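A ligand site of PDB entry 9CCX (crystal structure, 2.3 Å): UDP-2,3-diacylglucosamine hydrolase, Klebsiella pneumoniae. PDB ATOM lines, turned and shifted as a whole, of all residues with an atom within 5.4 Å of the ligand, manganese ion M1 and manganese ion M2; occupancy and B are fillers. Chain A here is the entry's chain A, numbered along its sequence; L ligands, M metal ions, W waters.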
ATOM      1  N   ASP A   8      36.379  19.174  -4.686  1.00  0.00           N
ATOM      2  CA  ASP A   8      35.823  20.511  -4.731  1.00  0.00           C
ATOM      3  C   ASP A   8      36.114  21.190  -6.061  1.00  0.00           C
ATOM      4  O   ASP A   8      36.510  22.354  -6.103  1.00  0.00           O
ATOM      5  CB  ASP A   8      36.347  21.357  -3.568  1.00  0.00           C
ATOM      6  CG  ASP A   8      35.806  20.888  -2.230  1.00  0.00           C
ATOM      7  OD1 ASP A   8      34.595  20.988  -2.000  1.00  0.00           O
ATOM      8  OD2 ASP A   8      36.586  20.388  -1.398  1.00  0.00           O
ATOM      9  N   HIS A  10      33.660  21.337  -8.488  1.00  0.00           N
ATOM     10  CA  HIS A  10      32.411  22.016  -8.826  1.00  0.00           C
ATOM     11  C   HIS A  10      32.222  22.170 -10.338  1.00  0.00           C
ATOM     12  O   HIS A  10      31.877  23.242 -10.834  1.00  0.00           O
ATOM     13  CB  HIS A  10      32.333  23.382  -8.137  1.00  0.00           C
ATOM     14  CG  HIS A  10      32.664  23.322  -6.686  1.00  0.00           C
ATOM     15  ND1 HIS A  10      33.842  23.812  -6.167  1.00  0.00           N
ATOM     16  CD2 HIS A  10      31.974  22.819  -5.635  1.00  0.00           C
ATOM     17  CE1 HIS A  10      33.861  23.622  -4.864  1.00  0.00           C
ATOM     18  NE2 HIS A  10      32.740  23.009  -4.510  1.00  0.00           N
ATOM     19  N   ASP A  41      32.223  16.815  -4.130  1.00  0.00           N
ATOM     20  CA  ASP A  41      32.050  18.077  -4.856  1.00  0.00           C
ATOM     21  C   ASP A  41      32.753  18.040  -6.215  1.00  0.00           C
ATOM     22  O   ASP A  41      33.303  19.054  -6.683  1.00  0.00           O
ATOM     23  CB  ASP A  41      32.524  19.298  -4.047  1.00  0.00           C
ATOM     24  CG  ASP A  41      31.525  19.749  -2.978  1.00  0.00           C
ATOM     25  OD1 ASP A  41      30.480  19.064  -2.791  1.00  0.00           O
ATOM     26  OD2 ASP A  41      31.787  20.790  -2.329  1.00  0.00           O
ATOM     27  N   GLU A  44      29.095  20.685  -9.475  1.00  0.00           N
ATOM     28  CA  GLU A  44      28.429  21.769  -8.760  1.00  0.00           C
ATOM     29  C   GLU A  44      27.014  21.393  -8.322  1.00  0.00           C
ATOM     30  O   GLU A  44      26.493  21.965  -7.352  1.00  0.00           O
ATOM     31  CB  GLU A  44      28.406  23.039  -9.628  1.00  0.00           C
ATOM     32  CG  GLU A  44      27.537  24.177  -9.094  1.00  0.00           C
ATOM     33  CD  GLU A  44      28.209  24.946  -7.968  1.00  0.00           C
ATOM     34  OE1 GLU A  44      29.245  24.461  -7.448  1.00  0.00           O
ATOM     35  OE2 GLU A  44      27.684  26.013  -7.570  1.00  0.00           O
ATOM     36  N   ALA A  45      26.386  20.449  -9.009  1.00  0.00           N
ATOM     37  CA  ALA A  45      25.039  20.019  -8.681  1.00  0.00           C
ATOM     38  C   ALA A  45      24.813  18.609  -9.210  1.00  0.00           C
ATOM     39  O   ALA A  45      25.524  18.146 -10.107  1.00  0.00           O
ATOM     40  CB  ALA A  45      23.972  20.978  -9.260  1.00  0.00           C
ATOM     41  N   TRP A  46      23.840  17.930  -8.622  1.00  0.00           N
ATOM     42  CA  TRP A  46      23.471  16.602  -9.107  1.00  0.00           C
ATOM     43  C   TRP A  46      22.042  16.310  -8.676  1.00  0.00           C
ATOM     44  O   TRP A  46      21.700  16.471  -7.508  1.00  0.00           O
ATOM     45  CB  TRP A  46      24.421  15.529  -8.574  1.00  0.00           C
ATOM     46  CG  TRP A  46      24.382  14.232  -9.333  1.00  0.00           C
ATOM     47  CD1 TRP A  46      23.570  13.154  -9.082  1.00  0.00           C
ATOM     48  CD2 TRP A  46      25.185  13.878 -10.470  1.00  0.00           C
ATOM     49  NE1 TRP A  46      23.833  12.151 -10.001  1.00  0.00           N
ATOM     50  CE2 TRP A  46      24.822  12.572 -10.855  1.00  0.00           C
ATOM     51  CE3 TRP A  46      26.198  14.534 -11.184  1.00  0.00           C
ATOM     52  CZ2 TRP A  46      25.431  11.904 -11.920  1.00  0.00           C
ATOM     53  CZ3 TRP A  46      26.796  13.872 -12.259  1.00  0.00           C
ATOM     54  CH2 TRP A  46      26.417  12.575 -12.602  1.00  0.00           C
ATOM     55  N   ILE A  47      21.198  15.905  -9.634  1.00  0.00           N
ATOM     56  CA  ILE A  47      19.804  15.609  -9.338  1.00  0.00           C
ATOM     57  C   ILE A  47      19.440  14.177  -9.709  1.00  0.00           C
ATOM     58  O   ILE A  47      18.260  13.837  -9.782  1.00  0.00           O
ATOM     59  CB  ILE A  47      18.855  16.609 -10.023  1.00  0.00           C
ATOM     60  CG1 ILE A  47      19.031  16.585 -11.539  1.00  0.00           C
ATOM     61  CG2 ILE A  47      19.082  18.007  -9.475  1.00  0.00           C
ATOM     62  CD1 ILE A  47      17.917  17.264 -12.307  1.00  0.00           C
ATOM     63  N   GLY A  78      30.222  14.582  -1.870  1.00  0.00           N
ATOM     64  CA  GLY A  78      30.295  15.893  -1.271  1.00  0.00           C
ATOM     65  C   GLY A  78      28.917  16.381  -0.890  1.00  0.00           C
ATOM     66  O   GLY A  78      27.911  15.694  -1.039  1.00  0.00           O
ATOM     67  N   ASN A  79      28.879  17.611  -0.361  1.00  0.00           N
ATOM     68  CA  ASN A  79      27.580  18.173  -0.032  1.00  0.00           C
ATOM     69  C   ASN A  79      26.819  18.621  -1.274  1.00  0.00           C
ATOM     70  O   ASN A  79      25.590  18.685  -1.234  1.00  0.00           O
ATOM     71  CB  ASN A  79      27.719  19.337   0.964  1.00  0.00           C
ATOM     72  CG  ASN A  79      28.485  20.519   0.399  1.00  0.00           C
ATOM     73  OD1 ASN A  79      29.672  20.417   0.091  1.00  0.00           O
ATOM     74  ND2 ASN A  79      27.819  21.669   0.312  1.00  0.00           N
ATOM     75  N   ARG A  80      27.520  18.884  -2.377  1.00  0.00           N
ATOM     76  CA  ARG A  80      26.835  19.289  -3.609  1.00  0.00           C
ATOM     77  C   ARG A  80      26.359  18.111  -4.444  1.00  0.00           C
ATOM     78  O   ARG A  80      25.288  18.179  -5.047  1.00  0.00           O
ATOM     79  CB  ARG A  80      27.751  20.180  -4.469  1.00  0.00           C
ATOM     80  CG  ARG A  80      28.322  21.387  -3.759  1.00  0.00           C
ATOM     81  CD  ARG A  80      27.236  22.360  -3.313  1.00  0.00           C
ATOM     82  NE  ARG A  80      26.470  22.850  -4.447  1.00  0.00           N
ATOM     83  CZ  ARG A  80      25.613  23.862  -4.391  1.00  0.00           C
ATOM     84  NH1 ARG A  80      25.404  24.531  -3.266  1.00  0.00           N
ATOM     85  NH2 ARG A  80      24.944  24.202  -5.487  1.00  0.00           N
ATOM     86  N   PHE A  82      25.837  14.728  -3.517  1.00  0.00           N
ATOM     87  CA  PHE A  82      25.523  13.553  -2.700  1.00  0.00           C
ATOM     88  C   PHE A  82      24.549  12.583  -3.384  1.00  0.00           C
ATOM     89  O   PHE A  82      24.324  11.494  -2.857  1.00  0.00           O
ATOM     90  CB  PHE A  82      24.961  13.995  -1.335  1.00  0.00           C
ATOM     91  CG  PHE A  82      23.693  14.828  -1.432  1.00  0.00           C
ATOM     92  CD1 PHE A  82      22.447  14.212  -1.437  1.00  0.00           C
ATOM     93  CD2 PHE A  82      23.759  16.206  -1.514  1.00  0.00           C
ATOM     94  CE1 PHE A  82      21.284  14.954  -1.549  1.00  0.00           C
ATOM     95  CE2 PHE A  82      22.595  16.962  -1.607  1.00  0.00           C
ATOM     96  CZ  PHE A  82      21.358  16.329  -1.634  1.00  0.00           C
ATOM     97  N   LEU A  83      23.964  12.947  -4.529  1.00  0.00           N
ATOM     98  CA  LEU A  83      23.068  12.028  -5.211  1.00  0.00           C
ATOM     99  C   LEU A  83      23.775  11.194  -6.292  1.00  0.00           C
ATOM    100  O   LEU A  83      23.113  10.423  -6.990  1.00  0.00           O
ATOM    101  CB  LEU A  83      21.886  12.787  -5.834  1.00  0.00           C
ATOM    102  CG  LEU A  83      20.779  13.348  -4.931  1.00  0.00           C
ATOM    103  CD1 LEU A  83      19.654  13.962  -5.757  1.00  0.00           C
ATOM    104  CD2 LEU A  83      20.220  12.306  -3.955  1.00  0.00           C
ATOM    105  N   HIS A 114      34.865  13.932   3.019  1.00  0.00           N
ATOM    106  CA  HIS A 114      34.658  15.210   2.341  1.00  0.00           C
ATOM    107  C   HIS A 114      34.958  16.383   3.266  1.00  0.00           C
ATOM    108  O   HIS A 114      35.519  17.396   2.833  1.00  0.00           O
ATOM    109  CB  HIS A 114      33.225  15.328   1.807  1.00  0.00           C
ATOM    110  CG  HIS A 114      32.974  16.616   1.082  1.00  0.00           C
ATOM    111  ND1 HIS A 114      33.679  16.989  -0.039  1.00  0.00           N
ATOM    112  CD2 HIS A 114      32.122  17.643   1.349  1.00  0.00           C
ATOM    113  CE1 HIS A 114      33.258  18.170  -0.455  1.00  0.00           C
ATOM    114  NE2 HIS A 114      32.323  18.600   0.379  1.00  0.00           N
ATOM    115  N   ASP A 116      32.493  17.949   5.315  1.00  0.00           N
ATOM    116  CA  ASP A 116      31.375  18.794   5.716  1.00  0.00           C
ATOM    117  C   ASP A 116      30.833  18.385   7.083  1.00  0.00           C
ATOM    118  O   ASP A 116      30.304  19.235   7.817  1.00  0.00           O
ATOM    119  CB  ASP A 116      30.263  18.811   4.657  1.00  0.00           C
ATOM    120  CG  ASP A 116      29.645  17.448   4.426  1.00  0.00           C
ATOM    121  OD1 ASP A 116      30.401  16.457   4.270  1.00  0.00           O
ATOM    122  OD2 ASP A 116      28.393  17.368   4.400  1.00  0.00           O
ATOM    123  N   TYR A 125      23.442  24.460   8.391  1.00  0.00           N
ATOM    124  CA  TYR A 125      23.834  23.464   7.408  1.00  0.00           C
ATOM    125  C   TYR A 125      23.483  22.059   7.866  1.00  0.00           C
ATOM    126  O   TYR A 125      22.996  21.239   7.073  1.00  0.00           O
ATOM    127  CB  TYR A 125      25.326  23.549   7.085  1.00  0.00           C
ATOM    128  CG  TYR A 125      25.756  22.358   6.256  1.00  0.00           C
ATOM    129  CD1 TYR A 125      25.249  22.184   4.974  1.00  0.00           C
ATOM    130  CD2 TYR A 125      26.667  21.427   6.735  1.00  0.00           C
ATOM    131  CE1 TYR A 125      25.599  21.092   4.193  1.00  0.00           C
ATOM    132  CE2 TYR A 125      27.044  20.338   5.963  1.00  0.00           C
ATOM    133  CZ  TYR A 125      26.502  20.178   4.692  1.00  0.00           C
ATOM    134  OH  TYR A 125      26.848  19.103   3.916  1.00  0.00           O
ATOM    135  N   PHE A 128      19.873  21.266   7.135  1.00  0.00           N
ATOM    136  CA  PHE A 128      19.728  21.014   5.710  1.00  0.00           C
ATOM    137  C   PHE A 128      20.300  19.660   5.324  1.00  0.00           C
ATOM    138  O   PHE A 128      19.664  18.898   4.592  1.00  0.00           O
ATOM    139  CB  PHE A 128      20.397  22.152   4.925  1.00  0.00           C
ATOM    140  CG  PHE A 128      20.381  21.960   3.442  1.00  0.00           C
ATOM    141  CD1 PHE A 128      19.355  22.490   2.678  1.00  0.00           C
ATOM    142  CD2 PHE A 128      21.414  21.296   2.790  1.00  0.00           C
ATOM    143  CE1 PHE A 128      19.342  22.336   1.300  1.00  0.00           C
ATOM    144  CE2 PHE A 128      21.406  21.147   1.419  1.00  0.00           C
ATOM    145  CZ  PHE A 128      20.366  21.657   0.676  1.00  0.00           C
ATOM    146  N   LYS A 131      18.192  16.623   6.302  1.00  0.00           N
ATOM    147  CA  LYS A 131      16.999  16.534   5.473  1.00  0.00           C
ATOM    148  C   LYS A 131      17.292  15.789   4.178  1.00  0.00           C
ATOM    149  O   LYS A 131      16.738  14.713   3.926  1.00  0.00           O
ATOM    150  CB  LYS A 131      16.477  17.952   5.188  1.00  0.00           C
ATOM    151  CG  LYS A 131      15.039  18.071   4.707  1.00  0.00           C
ATOM    152  CD  LYS A 131      14.887  19.327   3.841  1.00  0.00           C
ATOM    153  CE  LYS A 131      14.795  20.582   4.701  1.00  0.00           C
ATOM    154  NZ  LYS A 131      15.537  21.729   4.066  1.00  0.00           N
ATOM    155  N   VAL A 132      18.193  16.339   3.345  1.00  0.00           N
ATOM    156  CA  VAL A 132      18.429  15.797   2.005  1.00  0.00           C
ATOM    157  C   VAL A 132      19.246  14.511   2.027  1.00  0.00           C
ATOM    158  O   VAL A 132      19.516  13.956   0.952  1.00  0.00           O
ATOM    159  CB  VAL A 132      19.155  16.823   1.115  1.00  0.00           C
ATOM    160  CG1 VAL A 132      18.307  18.065   0.941  1.00  0.00           C
ATOM    161  CG2 VAL A 132      20.540  17.162   1.663  1.00  0.00           C
ATOM    162  N   ILE A 137      13.412  10.698   1.739  1.00  0.00           N
ATOM    163  CA  ILE A 137      13.318  11.994   1.077  1.00  0.00           C
ATOM    164  C   ILE A 137      14.104  11.982  -0.227  1.00  0.00           C
ATOM    165  O   ILE A 137      13.686  12.609  -1.213  1.00  0.00           O
ATOM    166  CB  ILE A 137      13.783  13.115   2.021  1.00  0.00           C
ATOM    167  CG1 ILE A 137      12.861  13.181   3.250  1.00  0.00           C
ATOM    168  CG2 ILE A 137      13.854  14.456   1.289  1.00  0.00           C
ATOM    169  CD1 ILE A 137      13.069  14.386   4.128  1.00  0.00           C
ATOM    170  N   GLN A 138      15.241  11.288  -0.262  1.00  0.00           N
ATOM    171  CA  GLN A 138      15.994  11.150  -1.508  1.00  0.00           C
ATOM    172  C   GLN A 138      15.213  10.337  -2.532  1.00  0.00           C
ATOM    173  O   GLN A 138      15.124  10.725  -3.699  1.00  0.00           O
ATOM    174  CB  GLN A 138      17.359  10.485  -1.245  1.00  0.00           C
ATOM    175  CG  GLN A 138      18.296  11.306  -0.380  1.00  0.00           C
ATOM    176  CD  GLN A 138      19.677  10.701  -0.321  1.00  0.00           C
ATOM    177  OE1 GLN A 138      19.831   9.485  -0.427  1.00  0.00           O
ATOM    178  NE2 GLN A 138      20.700  11.545  -0.176  1.00  0.00           N
ATOM    179  N   PHE A 141      12.438  12.358  -4.008  1.00  0.00           N
ATOM    180  CA  PHE A 141      12.939  13.378  -4.924  1.00  0.00           C
ATOM    181  C   PHE A 141      13.350  12.747  -6.241  1.00  0.00           C
ATOM    182  O   PHE A 141      12.971  13.237  -7.320  1.00  0.00           O
ATOM    183  CB  PHE A 141      14.099  14.147  -4.284  1.00  0.00           C
ATOM    184  CG  PHE A 141      14.764  15.134  -5.207  1.00  0.00           C
ATOM    185  CD1 PHE A 141      14.209  16.398  -5.403  1.00  0.00           C
ATOM    186  CD2 PHE A 141      15.938  14.821  -5.859  1.00  0.00           C
ATOM    187  CE1 PHE A 141      14.820  17.320  -6.241  1.00  0.00           C
ATOM    188  CE2 PHE A 141      16.561  15.744  -6.692  1.00  0.00           C
ATOM    189  CZ  PHE A 141      15.990  16.990  -6.881  1.00  0.00           C
ATOM    190  N   ILE A 152      13.006  22.346  -8.733  1.00  0.00           N
ATOM    191  CA  ILE A 152      13.239  22.299  -7.287  1.00  0.00           C
ATOM    192  C   ILE A 152      14.668  22.695  -6.958  1.00  0.00           C
ATOM    193  O   ILE A 152      14.922  23.467  -6.028  1.00  0.00           O
ATOM    194  CB  ILE A 152      12.921  20.884  -6.749  1.00  0.00           C
ATOM    195  CG1 ILE A 152      11.447  20.586  -6.919  1.00  0.00           C
ATOM    196  CG2 ILE A 152      13.380  20.764  -5.281  1.00  0.00           C
ATOM    197  CD1 ILE A 152      11.086  19.154  -6.569  1.00  0.00           C
ATOM    198  N   ALA A 153      15.632  22.172  -7.724  1.00  0.00           N
ATOM    199  CA  ALA A 153      17.041  22.382  -7.397  1.00  0.00           C
ATOM    200  C   ALA A 153      17.468  23.820  -7.656  1.00  0.00           C
ATOM    201  O   ALA A 153      18.169  24.424  -6.836  1.00  0.00           O
ATOM    202  CB  ALA A 153      17.899  21.405  -8.211  1.00  0.00           C
ATOM    203  N   ALA A 154      17.057  24.386  -8.792  1.00  0.00           N
ATOM    204  CA  ALA A 154      17.346  25.787  -9.082  1.00  0.00           C
ATOM    205  C   ALA A 154      16.768  26.707  -8.024  1.00  0.00           C
ATOM    206  O   ALA A 154      17.389  27.713  -7.647  1.00  0.00           O
ATOM    207  CB  ALA A 154      16.806  26.163 -10.457  1.00  0.00           C
ATOM    208  N   MET A 156      16.168  25.826  -4.816  1.00  0.00           N
ATOM    209  CA  MET A 156      16.911  25.643  -3.573  1.00  0.00           C
ATOM    210  C   MET A 156      18.277  26.302  -3.636  1.00  0.00           C
ATOM    211  O   MET A 156      18.796  26.763  -2.608  1.00  0.00           O
ATOM    212  CB  MET A 156      17.046  24.163  -3.225  1.00  0.00           C
ATOM    213  CG  MET A 156      15.717  23.489  -2.884  1.00  0.00           C
ATOM    214  SD  MET A 156      15.903  21.700  -2.620  1.00  0.00           S
ATOM    215  CE  MET A 156      17.242  21.688  -1.416  1.00  0.00           C
ATOM    216  N   ARG A 157      18.868  26.384  -4.824  1.00  0.00           N
ATOM    217  CA  ARG A 157      20.162  27.051  -4.944  1.00  0.00           C
ATOM    218  C   ARG A 157      20.021  28.553  -4.698  1.00  0.00           C
ATOM    219  O   ARG A 157      20.850  29.148  -3.997  1.00  0.00           O
ATOM    220  CB  ARG A 157      20.764  26.772  -6.316  1.00  0.00           C
ATOM    221  CG  ARG A 157      21.297  25.341  -6.474  1.00  0.00           C
ATOM    222  CD  ARG A 157      22.202  25.195  -7.695  1.00  0.00           C
ATOM    223  NE  ARG A 157      21.488  25.404  -8.946  1.00  0.00           N
ATOM    224  CZ  ARG A 157      20.897  24.446  -9.644  1.00  0.00           C
ATOM    225  NH1 ARG A 157      20.895  23.188  -9.228  1.00  0.00           N
ATOM    226  NH2 ARG A 157      20.289  24.759 -10.796  1.00  0.00           N
ATOM    227  N   SER A 160      19.561  29.351  -1.005  1.00  0.00           N
ATOM    228  CA  SER A 160      20.774  29.277  -0.190  1.00  0.00           C
ATOM    229  C   SER A 160      21.677  30.487  -0.392  1.00  0.00           C
ATOM    230  O   SER A 160      22.300  30.941   0.582  1.00  0.00           O
ATOM    231  CB  SER A 160      21.548  27.992  -0.485  1.00  0.00           C
ATOM    232  OG  SER A 160      20.791  26.879  -0.047  1.00  0.00           O
ATOM    233  N   HIS A 195      36.054  20.331   1.158  1.00  0.00           N
ATOM    234  CA  HIS A 195      34.849  21.062   1.536  1.00  0.00           C
ATOM    235  C   HIS A 195      35.071  22.500   1.983  1.00  0.00           C
ATOM    236  O   HIS A 195      34.336  23.385   1.551  1.00  0.00           O
ATOM    237  CB  HIS A 195      34.083  20.351   2.643  1.00  0.00           C
ATOM    238  CG  HIS A 195      32.894  21.134   3.112  1.00  0.00           C
ATOM    239  ND1 HIS A 195      31.806  21.378   2.302  1.00  0.00           N
ATOM    240  CD2 HIS A 195      32.649  21.757   4.287  1.00  0.00           C
ATOM    241  CE1 HIS A 195      30.927  22.104   2.971  1.00  0.00           C
ATOM    242  NE2 HIS A 195      31.412  22.346   4.170  1.00  0.00           N
ATOM    243  N   HIS A 197      37.569  24.507   1.344  1.00  0.00           N
ATOM    244  CA  HIS A 197      38.234  25.334   0.338  1.00  0.00           C
ATOM    245  C   HIS A 197      39.402  26.138   0.925  1.00  0.00           C
ATOM    246  O   HIS A 197      39.772  27.192   0.402  1.00  0.00           O
ATOM    247  CB  HIS A 197      37.257  26.301  -0.363  1.00  0.00           C
ATOM    248  CG  HIS A 197      36.114  25.628  -1.073  1.00  0.00           C
ATOM    249  ND1 HIS A 197      35.184  26.344  -1.799  1.00  0.00           N
ATOM    250  CD2 HIS A 197      35.767  24.325  -1.194  1.00  0.00           C
ATOM    251  CE1 HIS A 197      34.295  25.508  -2.314  1.00  0.00           C
ATOM    252  NE2 HIS A 197      34.632  24.281  -1.965  1.00  0.00           N
HETATM  253  C1  LIG L   1      22.197  21.390  -4.262  1.00  0.00           C
HETATM  254  C2  LIG L   1      23.657  21.264  -2.347  1.00  0.00           C
HETATM  255  C3  LIG L   1      22.067  23.099  -2.566  1.00  0.00           C
HETATM  256  C4  LIG L   1      22.599  24.441  -0.620  1.00  0.00           C
HETATM  257  C5  LIG L   1      24.252  22.794   0.455  1.00  0.00           C
HETATM  258  C6  LIG L   1      24.432  23.683   1.681  1.00  0.00           C
HETATM  259  C7  LIG L   1      15.468  17.066  -2.000  1.00  0.00           C
HETATM  260  C8  LIG L   1      14.126  17.642  -1.576  1.00  0.00           C
HETATM  261  C9  LIG L   1      17.074  15.297  -2.028  1.00  0.00           C
HETATM  262  C10 LIG L   1      17.535  17.254  -3.160  1.00  0.00           C
HETATM  263  C11 LIG L   1      18.021  19.241  -4.640  1.00  0.00           C
HETATM  264  C12 LIG L   1      19.172  20.220  -4.758  1.00  0.00           C
HETATM  265  C13 LIG L   1      20.749  18.375  -4.709  1.00  0.00           C
HETATM  266  C14 LIG L   1      19.582  17.397  -4.609  1.00  0.00           C
HETATM  267  C15 LIG L   1      23.209  20.725  -3.550  1.00  0.00           C
HETATM  268  C16 LIG L   1      23.085  22.447  -1.852  1.00  0.00           C
HETATM  269  C17 LIG L   1      21.607  22.567  -3.780  1.00  0.00           C
HETATM  270  C18 LIG L   1      21.647  24.346  -1.778  1.00  0.00           C
HETATM  271  C19 LIG L   1      16.326  17.809  -2.786  1.00  0.00           C
HETATM  272  C20 LIG L   1      15.850  15.783  -1.615  1.00  0.00           C
HETATM  273  F1  LIG L   1      14.294  18.345  -0.437  1.00  0.00           F
HETATM  274  F2  LIG L   1      13.616  18.493  -2.534  1.00  0.00           F
HETATM  275  F3  LIG L   1      13.263  16.607  -1.364  1.00  0.00           F
HETATM  276  N1  LIG L   1      17.870  16.032  -2.787  1.00  0.00           N
HETATM  277  N2  LIG L   1      18.442  18.024  -3.965  1.00  0.00           N
HETATM  278  N3  LIG L   1      20.373  19.621  -5.350  1.00  0.00           N
HETATM  279  N4  LIG L   1      23.360  23.221  -0.607  1.00  0.00           N
HETATM  280  O1  LIG L   1      21.163  21.720  -6.758  1.00  0.00           O
HETATM  281  O2  LIG L   1      22.685  19.970  -6.541  1.00  0.00           O
HETATM  282  O3  LIG L   1      24.841  21.768   0.351  1.00  0.00           O
HETATM  283  S1  LIG L   1      21.623  20.676  -5.821  1.00  0.00           S
HETATM  284 MN    MN M   1      31.637  20.762  -0.021  1.00  0.00          MN
HETATM  285 MN    MN M   2      33.202  22.501  -2.324  1.00  0.00          MN
HETATM  286  O   HOH W   1      32.367  22.774  -0.330  1.00  0.00           O
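ND2 of Asn 79 is in hydrogen-bond range of O3 of the ligand (3.0 Å).
The guanidinium group (NH1) of Arg 157 lies within hydrogen-bond range of an oxygen (O1) of the ligand (2.9 Å).
N of Trp 46 lies within hydrogen-bond range of O2 of the ligand (3.1 Å).
An oxygen (O2) of the ligand sits close to the backbone carbonyl oxygen of Arg 80 (3.5 Å).
Ala 45 touches the ligand (CB to O2, 3.2 Å).
Phe 82 touches the ligand.
CD1 of Leu 83 touches C14 of the ligand, 3.6 Å away.
Tyr 125 touches the ligand.
CE2 of Phe 128 touches C5 of the ligand, at 3.4 Å.
Ile 137 touches the ligand.
CB of Phe 141 touches C20 of the ligand (3.6 Å).
CG2 of Ile 152 touches F2 of the ligand, at 3.6 Å.
CB of Ala 153 touches O1 of the ligand, at 3.6 Å.
Met 156 touches the ligand (SD to C11, 3.8 Å).
Ser 160 touches the ligand (OG to C4, 3.1 Å).
Of the 29 residues printed, 15 come within 4 Å of the ligand.
Along chain A the residues within 4 Å of the ligand span positions 45 to 160.
OD1 of Asp 8 binds manganese ion M2 (2.1 Å).
Water W1 binds manganese ion M2.
OD2 of Asp 41 is bound to manganese ion M2, at 2.2 Å.
Manganese ion M2 is bound by NE2 of His 10.
Manganese ion M2 is bound by a ring nitrogen (NE2) of His 197.
The backbone NH of His 195 sits at hydrogen-bond distance from the side-chain carboxylate of Asp 8.
OD1 of Asp 41 sits at hydrogen-bond distance from N of Arg 80.
OG of Ser 160 is in hydrogen-bond range of O of Met 156, 3.2 Å away.
The guanidinium group (NH2) of Arg 80 is in salt-bridge range of the side-chain carboxylate (OE2) of Glu 44.
Within 4 Å of manganese ion M2: Asp 8, His 10, Asp 41 and His 197.
The nearest printed residue that does not touch manganese ion M2 is His 195 (4.1 Å).
Manganese ion M1 is bound by OD1 of Asn 79, water W1, NE2 of His 114, OD2 of Asp 41 and ND1 of His 195.
Manganese ion M1 has five donor atoms within binding distance.
Within 4 Å of manganese ion M1: Asp 8, Asp 41, Asn 79, His 114 and His 195.
Along chain A the residues within 4 Å of manganese ion M1 span positions 8 to 195.
The nearest printed residue that does not touch manganese ion M1 is His 197 (5.0 Å).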
